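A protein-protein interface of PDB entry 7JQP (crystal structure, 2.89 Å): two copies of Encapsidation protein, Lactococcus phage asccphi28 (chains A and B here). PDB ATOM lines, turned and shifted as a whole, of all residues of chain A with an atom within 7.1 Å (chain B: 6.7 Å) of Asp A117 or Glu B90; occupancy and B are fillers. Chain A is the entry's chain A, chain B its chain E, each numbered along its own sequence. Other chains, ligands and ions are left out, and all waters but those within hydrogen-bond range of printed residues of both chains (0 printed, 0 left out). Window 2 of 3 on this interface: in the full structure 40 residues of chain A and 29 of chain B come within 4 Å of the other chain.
Among the printed residues, pairs that only touch across the chains: Phe A114 with Glu B90, Pro A138 with Asn B68, Phe A114 with Ser B91, Tyr A122 with Asn B68, Arg A118 with Glu B90 and Lys A107 with Ser B91.
No position is printed for both chains.
OD1 of Asp B89 sits close to OD2 of Asp A117, at 3.4 Å. The side-chain hydroxyl of Ser B91 is in hydrogen-bond range of the side-chain carboxylate of Asp A117, 3.0 Å away. N of Glu B90 is in hydrogen-bond range of O of Asp A117, 2.9 Å away. The backbone NH of Cys A119 is in hydrogen-bond range of the side-chain carboxylate of Glu B90 (2.8 Å).
Asp A117 touches just these residues of chain B: Asp B89 (3.0 Å), Glu B90 (2.9 Å) and Ser B91 (3.0 Å). Of chain A, only Phe A114, Asp A117, Arg A118 and Cys A119 come within 4 Å of Glu B90. Of the printed residues of chain B, Phe A114 touches Glu B90 (3.3 Å) and Ser B91 (3.5 Å). Of the printed residues of chain A, Asp B89 touches Asp A117. Of the printed residues of chain A, Asn B68 touches Tyr A122 (3.6 Å) and Pro A138 (3.4 Å). Printed residues of chain A within 4 Å of Ser B91: Lys A107, Phe A114 and Asp A117. Printed residues of chain B within 4 Å of Arg A118: Glu B90. Glu A105 touches none of the printed residues of chain B. Asp A116 touches none of the printed residues of chain B. The nearest printed residue of chain B that does not touch Phe A114 is Lys B92 (5.6 Å).
Among the printed residues, no Asp or Glu carboxylate lies within 4 Å of a Lys or Arg side-chain nitrogen of the other chain.
N of Ser B91 sits close to OD1 of Asp B89 (3.3 Å). The side-chain hydroxyl of Ser A50 sits at hydrogen-bond distance from the backbone carbonyl oxygen of Cys A119 (3.0 Å). N of Asp B89 is in hydrogen-bond range of O of Ile B94, 2.9 Å away. The side-chain carboxylate (OE2) of Glu A105 lies within salt-bridge range of the side-chain amino group (NZ) of Lys A107, 3.7 Å away. The backbone carbonyl oxygen (O) of Ile A113 lies close to the side-chain sulfur (SG) of Cys A119, at 3.8 Å. O of Lys A107 lies within hydrogen-bond range of N of Phe A114, at 2.5 Å.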
ATOM      1  N   ASN A  48      -5.635  -7.758 -22.692  1.00  0.00           N
ATOM      2  CA  ASN A  48      -5.023  -7.381 -23.968  1.00  0.00           C
ATOM      3  C   ASN A  48      -5.635  -6.100 -24.528  1.00  0.00           C
ATOM      4  O   ASN A  48      -5.846  -5.967 -25.736  1.00  0.00           O
ATOM      5  CB  ASN A  48      -5.139  -8.519 -24.985  1.00  0.00           C
ATOM      6  CG  ASN A  48      -3.810  -8.877 -25.618  1.00  0.00           C
ATOM      7  OD1 ASN A  48      -3.000  -9.587 -25.022  1.00  0.00           O
ATOM      8  ND2 ASN A  48      -3.579  -8.387 -26.831  1.00  0.00           N
ATOM      9  N   SER A  50      -5.314  -1.736 -24.335  1.00  0.00           N
ATOM     10  CA  SER A  50      -4.438  -0.633 -23.980  1.00  0.00           C
ATOM     11  C   SER A  50      -5.271   0.525 -23.445  1.00  0.00           C
ATOM     12  O   SER A  50      -6.503   0.515 -23.479  1.00  0.00           O
ATOM     13  CB  SER A  50      -3.609  -0.185 -25.188  1.00  0.00           C
ATOM     14  OG  SER A  50      -2.882  -1.268 -25.740  1.00  0.00           O
ATOM     15  N   GLU A 105       6.162  -7.092 -15.054  1.00  0.00           N
ATOM     16  CA  GLU A 105       7.048  -5.939 -14.954  1.00  0.00           C
ATOM     17  C   GLU A 105       6.425  -4.775 -15.710  1.00  0.00           C
ATOM     18  O   GLU A 105       5.977  -4.939 -16.851  1.00  0.00           O
ATOM     19  CB  GLU A 105       8.455  -6.272 -15.479  1.00  0.00           C
ATOM     20  CG  GLU A 105       8.698  -6.059 -16.961  1.00  0.00           C
ATOM     21  CD  GLU A 105      10.185  -6.018 -17.295  1.00  0.00           C
ATOM     22  OE1 GLU A 105      11.002  -6.399 -16.426  1.00  0.00           O
ATOM     23  OE2 GLU A 105      10.536  -5.603 -18.419  1.00  0.00           O
ATOM     24  N   LYS A 107       7.210  -1.196 -17.296  1.00  0.00           N
ATOM     25  CA  LYS A 107       8.293  -0.377 -17.828  1.00  0.00           C
ATOM     26  C   LYS A 107       7.704   0.845 -18.508  1.00  0.00           C
ATOM     27  O   LYS A 107       6.807   0.718 -19.347  1.00  0.00           O
ATOM     28  CB  LYS A 107       9.126  -1.215 -18.801  1.00  0.00           C
ATOM     29  CG  LYS A 107      10.230  -0.493 -19.543  1.00  0.00           C
ATOM     30  CD  LYS A 107      10.760  -1.373 -20.687  1.00  0.00           C
ATOM     31  CE  LYS A 107      11.063  -2.795 -20.214  1.00  0.00           C
ATOM     32  NZ  LYS A 107      11.771  -3.595 -21.256  1.00  0.00           N
ATOM     33  N   LYS A 112       4.993   6.144 -23.414  1.00  0.00           N
ATOM     34  CA  LYS A 112       4.296   4.873 -23.316  1.00  0.00           C
ATOM     35  C   LYS A 112       4.662   4.181 -22.010  1.00  0.00           C
ATOM     36  O   LYS A 112       5.757   4.367 -21.475  1.00  0.00           O
ATOM     37  CB  LYS A 112       4.655   3.957 -24.496  1.00  0.00           C
ATOM     38  CG  LYS A 112       4.335   4.548 -25.859  1.00  0.00           C
ATOM     39  CD  LYS A 112       4.624   3.558 -26.976  1.00  0.00           C
ATOM     40  CE  LYS A 112       4.324   4.162 -28.340  1.00  0.00           C
ATOM     41  NZ  LYS A 112       4.492   3.173 -29.441  1.00  0.00           N
ATOM     42  N   ILE A 113       3.738   3.364 -21.516  1.00  0.00           N
ATOM     43  CA  ILE A 113       3.974   2.474 -20.386  1.00  0.00           C
ATOM     44  C   ILE A 113       3.768   1.054 -20.891  1.00  0.00           C
ATOM     45  O   ILE A 113       2.760   0.770 -21.548  1.00  0.00           O
ATOM     46  CB  ILE A 113       3.022   2.776 -19.217  1.00  0.00           C
ATOM     47  CG1 ILE A 113       3.393   4.098 -18.548  1.00  0.00           C
ATOM     48  CG2 ILE A 113       3.080   1.635 -18.205  1.00  0.00           C
ATOM     49  CD1 ILE A 113       2.391   4.548 -17.502  1.00  0.00           C
ATOM     50  N   PHE A 114       4.716   0.170 -20.598  1.00  0.00           N
ATOM     51  CA  PHE A 114       4.686  -1.195 -21.104  1.00  0.00           C
ATOM     52  C   PHE A 114       4.500  -2.159 -19.941  1.00  0.00           C
ATOM     53  O   PHE A 114       5.169  -2.032 -18.910  1.00  0.00           O
ATOM     54  CB  PHE A 114       5.968  -1.525 -21.867  1.00  0.00           C
ATOM     55  CG  PHE A 114       6.212  -0.638 -23.052  1.00  0.00           C
ATOM     56  CD1 PHE A 114       6.870   0.569 -22.895  1.00  0.00           C
ATOM     57  CD2 PHE A 114       5.768  -0.994 -24.314  1.00  0.00           C
ATOM     58  CE1 PHE A 114       7.099   1.398 -23.976  1.00  0.00           C
ATOM     59  CE2 PHE A 114       5.990  -0.165 -25.401  1.00  0.00           C
ATOM     60  CZ  PHE A 114       6.657   1.032 -25.231  1.00  0.00           C
ATOM     61  N   PHE A 115       3.597  -3.119 -20.116  1.00  0.00           N
ATOM     62  CA  PHE A 115       3.343  -4.178 -19.145  1.00  0.00           C
ATOM     63  C   PHE A 115       3.684  -5.506 -19.805  1.00  0.00           C
ATOM     64  O   PHE A 115       3.007  -5.924 -20.751  1.00  0.00           O
ATOM     65  CB  PHE A 115       1.887  -4.147 -18.683  1.00  0.00           C
ATOM     66  CG  PHE A 115       1.484  -5.329 -17.852  1.00  0.00           C
ATOM     67  CD1 PHE A 115       1.682  -5.328 -16.483  1.00  0.00           C
ATOM     68  CD2 PHE A 115       0.894  -6.436 -18.438  1.00  0.00           C
ATOM     69  CE1 PHE A 115       1.306  -6.408 -15.715  1.00  0.00           C
ATOM     70  CE2 PHE A 115       0.518  -7.522 -17.672  1.00  0.00           C
ATOM     71  CZ  PHE A 115       0.725  -7.507 -16.310  1.00  0.00           C
ATOM     72  N   ASP A 116       4.740  -6.162 -19.322  1.00  0.00           N
ATOM     73  CA  ASP A 116       5.168  -7.445 -19.885  1.00  0.00           C
ATOM     74  C   ASP A 116       5.424  -7.307 -21.383  1.00  0.00           C
ATOM     75  O   ASP A 116       4.972  -8.118 -22.194  1.00  0.00           O
ATOM     76  CB  ASP A 116       4.118  -8.515 -19.587  1.00  0.00           C
ATOM     77  CG  ASP A 116       4.212  -9.036 -18.170  1.00  0.00           C
ATOM     78  OD1 ASP A 116       4.764  -8.307 -17.319  1.00  0.00           O
ATOM     79  OD2 ASP A 116       3.647 -10.111 -17.883  1.00  0.00           O
ATOM     80  N   ASP A 117       6.155  -6.253 -21.747  1.00  0.00           N
ATOM     81  CA  ASP A 117       6.556  -5.974 -23.123  1.00  0.00           C
ATOM     82  C   ASP A 117       5.386  -5.591 -24.017  1.00  0.00           C
ATOM     83  O   ASP A 117       5.501  -5.652 -25.245  1.00  0.00           O
ATOM     84  CB  ASP A 117       7.298  -7.171 -23.735  1.00  0.00           C
ATOM     85  CG  ASP A 117       8.698  -7.346 -23.180  1.00  0.00           C
ATOM     86  OD1 ASP A 117       9.167  -6.441 -22.459  1.00  0.00           O
ATOM     87  OD2 ASP A 117       9.317  -8.399 -23.441  1.00  0.00           O
ATOM     88  N   ARG A 118       4.266  -5.170 -23.435  1.00  0.00           N
ATOM     89  CA  ARG A 118       3.104  -4.740 -24.204  1.00  0.00           C
ATOM     90  C   ARG A 118       2.644  -3.385 -23.691  1.00  0.00           C
ATOM     91  O   ARG A 118       2.366  -3.231 -22.497  1.00  0.00           O
ATOM     92  CB  ARG A 118       1.963  -5.757 -24.111  1.00  0.00           C
ATOM     93  CG  ARG A 118       0.731  -5.368 -24.915  1.00  0.00           C
ATOM     94  CD  ARG A 118      -0.346  -6.436 -24.826  1.00  0.00           C
ATOM     95  NE  ARG A 118      -0.638  -6.780 -23.437  1.00  0.00           N
ATOM     96  CZ  ARG A 118      -1.559  -6.179 -22.687  1.00  0.00           C
ATOM     97  NH1 ARG A 118      -2.296  -5.195 -23.185  1.00  0.00           N
ATOM     98  NH2 ARG A 118      -1.741  -6.569 -21.433  1.00  0.00           N
ATOM     99  N   CYS A 119       2.550  -2.414 -24.593  1.00  0.00           N
ATOM    100  CA  CYS A 119       2.115  -1.079 -24.209  1.00  0.00           C
ATOM    101  C   CYS A 119       0.686  -1.122 -23.686  1.00  0.00           C
ATOM    102  O   CYS A 119      -0.218  -1.628 -24.356  1.00  0.00           O
ATOM    103  CB  CYS A 119       2.205  -0.131 -25.403  1.00  0.00           C
ATOM    104  SG  CYS A 119       1.653   1.551 -25.051  1.00  0.00           S
ATOM    105  N   ILE A 120       0.490  -0.584 -22.486  1.00  0.00           N
ATOM    106  CA  ILE A 120      -0.831  -0.537 -21.876  1.00  0.00           C
ATOM    107  C   ILE A 120      -1.342   0.882 -21.685  1.00  0.00           C
ATOM    108  O   ILE A 120      -2.555   1.065 -21.496  1.00  0.00           O
ATOM    109  CB  ILE A 120      -0.844  -1.285 -20.526  1.00  0.00           C
ATOM    110  CG1 ILE A 120       0.312  -0.803 -19.646  1.00  0.00           C
ATOM    111  CG2 ILE A 120      -0.766  -2.788 -20.753  1.00  0.00           C
ATOM    112  CD1 ILE A 120       0.116  -1.082 -18.170  1.00  0.00           C
ATOM    113  N   TYR A 122      -0.951   4.999 -23.286  1.00  0.00           N
ATOM    114  CA  TYR A 122      -0.433   5.971 -24.235  1.00  0.00           C
ATOM    115  C   TYR A 122      -0.694   7.364 -23.678  1.00  0.00           C
ATOM    116  O   TYR A 122      -1.785   7.641 -23.167  1.00  0.00           O
ATOM    117  CB  TYR A 122      -1.105   5.889 -25.615  1.00  0.00           C
ATOM    118  CG  TYR A 122      -0.916   4.624 -26.418  1.00  0.00           C
ATOM    119  CD1 TYR A 122      -1.693   3.502 -26.177  1.00  0.00           C
ATOM    120  CD2 TYR A 122      -0.002   4.574 -27.466  1.00  0.00           C
ATOM    121  CE1 TYR A 122      -1.540   2.353 -26.928  1.00  0.00           C
ATOM    122  CE2 TYR A 122       0.158   3.431 -28.223  1.00  0.00           C
ATOM    123  CZ  TYR A 122      -0.614   2.324 -27.952  1.00  0.00           C
ATOM    124  OH  TYR A 122      -0.458   1.183 -28.708  1.00  0.00           O
ATOM    125  N   PRO A 138      -3.903  -0.095 -31.648  1.00  0.00           N
ATOM    126  CA  PRO A 138      -4.660  -1.325 -31.953  1.00  0.00           C
ATOM    127  C   PRO A 138      -5.801  -1.658 -30.999  1.00  0.00           C
ATOM    128  O   PRO A 138      -6.931  -1.858 -31.469  1.00  0.00           O
ATOM    129  CB  PRO A 138      -3.564  -2.410 -31.938  1.00  0.00           C
ATOM    130  CG  PRO A 138      -2.290  -1.671 -32.223  1.00  0.00           C
ATOM    131  CD  PRO A 138      -2.453  -0.342 -31.542  1.00  0.00           C
ATOM    132  N   ASP A 139      -5.555  -1.776 -29.696  1.00  0.00           N
ATOM    133  CA  ASP A 139      -6.552  -2.338 -28.775  1.00  0.00           C
ATOM    134  C   ASP A 139      -6.853  -1.419 -27.593  1.00  0.00           C
ATOM    135  O   ASP A 139      -6.773  -1.821 -26.427  1.00  0.00           O
ATOM    136  CB  ASP A 139      -6.124  -3.725 -28.303  1.00  0.00           C
ATOM    137  CG  ASP A 139      -5.898  -4.686 -29.460  1.00  0.00           C
ATOM    138  OD1 ASP A 139      -6.612  -4.572 -30.481  1.00  0.00           O
ATOM    139  OD2 ASP A 139      -5.011  -5.559 -29.350  1.00  0.00           O
ATOM    140  N   ASN B  67       6.006   2.717 -34.765  1.00  0.00           N
ATOM    141  CA  ASN B  67       5.901   1.312 -34.391  1.00  0.00           C
ATOM    142  C   ASN B  67       4.616   0.705 -34.941  1.00  0.00           C
ATOM    143  O   ASN B  67       4.598  -0.459 -35.358  1.00  0.00           O
ATOM    144  CB  ASN B  67       5.921   1.161 -32.872  1.00  0.00           C
ATOM    145  CG  ASN B  67       6.226  -0.259 -32.427  1.00  0.00           C
ATOM    146  OD1 ASN B  67       6.665  -1.092 -33.220  1.00  0.00           O
ATOM    147  ND2 ASN B  67       5.911  -0.564 -31.172  1.00  0.00           N
ATOM    148  N   ASN B  68       3.527   1.474 -34.936  1.00  0.00           N
ATOM    149  CA  ASN B  68       2.238   0.981 -35.394  1.00  0.00           C
ATOM    150  C   ASN B  68       1.950   1.333 -36.848  1.00  0.00           C
ATOM    151  O   ASN B  68       0.807   1.189 -37.295  1.00  0.00           O
ATOM    152  CB  ASN B  68       1.101   1.486 -34.503  1.00  0.00           C
ATOM    153  CG  ASN B  68       1.285   1.090 -33.053  1.00  0.00           C
ATOM    154  OD1 ASN B  68       2.219   0.366 -32.712  1.00  0.00           O
ATOM    155  ND2 ASN B  68       0.327   1.463 -32.213  1.00  0.00           N
ATOM    156  N   ALA B  88       5.221 -10.388 -30.401  1.00  0.00           N
ATOM    157  CA  ALA B  88       5.798  -9.058 -30.532  1.00  0.00           C
ATOM    158  C   ALA B  88       6.218  -8.503 -29.181  1.00  0.00           C
ATOM    159  O   ALA B  88       5.560  -8.744 -28.166  1.00  0.00           O
ATOM    160  CB  ALA B  88       4.807  -8.085 -31.193  1.00  0.00           C
ATOM    161  N   ASP B  89       7.318  -7.748 -29.187  1.00  0.00           N
ATOM    162  CA  ASP B  89       7.834  -7.048 -28.012  1.00  0.00           C
ATOM    163  C   ASP B  89       7.690  -5.551 -28.271  1.00  0.00           C
ATOM    164  O   ASP B  89       8.561  -4.932 -28.892  1.00  0.00           O
ATOM    165  CB  ASP B  89       9.288  -7.428 -27.745  1.00  0.00           C
ATOM    166  CG  ASP B  89       9.918  -6.592 -26.644  1.00  0.00           C
ATOM    167  OD1 ASP B  89       9.174  -6.011 -25.827  1.00  0.00           O
ATOM    168  OD2 ASP B  89      11.163  -6.508 -26.600  1.00  0.00           O
ATOM    169  N   GLU B  90       6.590  -4.968 -27.790  1.00  0.00           N
ATOM    170  CA  GLU B  90       6.324  -3.560 -28.068  1.00  0.00           C
ATOM    171  C   GLU B  90       7.337  -2.647 -27.389  1.00  0.00           C
ATOM    172  O   GLU B  90       7.659  -1.578 -27.921  1.00  0.00           O
ATOM    173  CB  GLU B  90       4.903  -3.200 -27.630  1.00  0.00           C
ATOM    174  CG  GLU B  90       3.816  -3.984 -28.358  1.00  0.00           C
ATOM    175  CD  GLU B  90       2.420  -3.441 -28.102  1.00  0.00           C
ATOM    176  OE1 GLU B  90       2.292  -2.424 -27.391  1.00  0.00           O
ATOM    177  OE2 GLU B  90       1.448  -4.034 -28.617  1.00  0.00           O
ATOM    178  N   SER B  91       7.853  -3.046 -26.224  1.00  0.00           N
ATOM    179  CA  SER B  91       8.800  -2.197 -25.508  1.00  0.00           C
ATOM    180  C   SER B  91      10.040  -1.918 -26.347  1.00  0.00           C
ATOM    181  O   SER B  91      10.561  -0.796 -26.344  1.00  0.00           O
ATOM    182  CB  SER B  91       9.181  -2.849 -24.180  1.00  0.00           C
ATOM    183  OG  SER B  91       9.607  -4.186 -24.374  1.00  0.00           O
ATOM    184  N   LYS B  92      10.529  -2.921 -27.073  1.00  0.00           N
ATOM    185  CA  LYS B  92      11.687  -2.756 -27.940  1.00  0.00           C
ATOM    186  C   LYS B  92      11.298  -2.570 -29.400  1.00  0.00           C
ATOM    187  O   LYS B  92      12.171  -2.596 -30.272  1.00  0.00           O
ATOM    188  CB  LYS B  92      12.633  -3.948 -27.784  1.00  0.00           C
ATOM    189  CG  LYS B  92      13.254  -4.038 -26.392  1.00  0.00           C
ATOM    190  CD  LYS B  92      14.364  -5.077 -26.309  1.00  0.00           C
ATOM    191  CE  LYS B  92      15.634  -4.599 -27.000  1.00  0.00           C
ATOM    192  NZ  LYS B  92      16.766  -5.550 -26.806  1.00  0.00           N
ATOM    193  N   GLN B  93      10.010  -2.375 -29.682  1.00  0.00           N
ATOM    194  CA  GLN B  93       9.532  -2.066 -31.029  1.00  0.00           C
ATOM    195  C   GLN B  93       9.940  -3.145 -32.030  1.00  0.00           C
ATOM    196  O   GLN B  93      10.405  -2.858 -33.135  1.00  0.00           O
ATOM    197  CB  GLN B  93      10.040  -0.691 -31.480  1.00  0.00           C
ATOM    198  CG  GLN B  93       9.331   0.483 -30.827  1.00  0.00           C
ATOM    199  CD  GLN B  93       9.795   1.828 -31.360  1.00  0.00           C
ATOM    200  OE1 GLN B  93      10.941   1.982 -31.779  1.00  0.00           O
ATOM    201  NE2 GLN B  93       8.899   2.808 -31.346  1.00  0.00           N
ATOM    202  N   ILE B  94       9.743  -4.403 -31.643  1.00  0.00           N
ATOM    203  CA  ILE B  94      10.089  -5.544 -32.483  1.00  0.00           C
ATOM    204  C   ILE B  94       8.838  -6.381 -32.714  1.00  0.00           C
ATOM    205  O   ILE B  94       8.083  -6.654 -31.773  1.00  0.00           O
ATOM    206  CB  ILE B  94      11.214  -6.396 -31.861  1.00  0.00           C
ATOM    207  CG1 ILE B  94      12.433  -5.515 -31.573  1.00  0.00           C
ATOM    208  CG2 ILE B  94      11.602  -7.536 -32.792  1.00  0.00           C
ATOM    209  CD1 ILE B  94      13.655  -6.265 -31.076  1.00  0.00           C
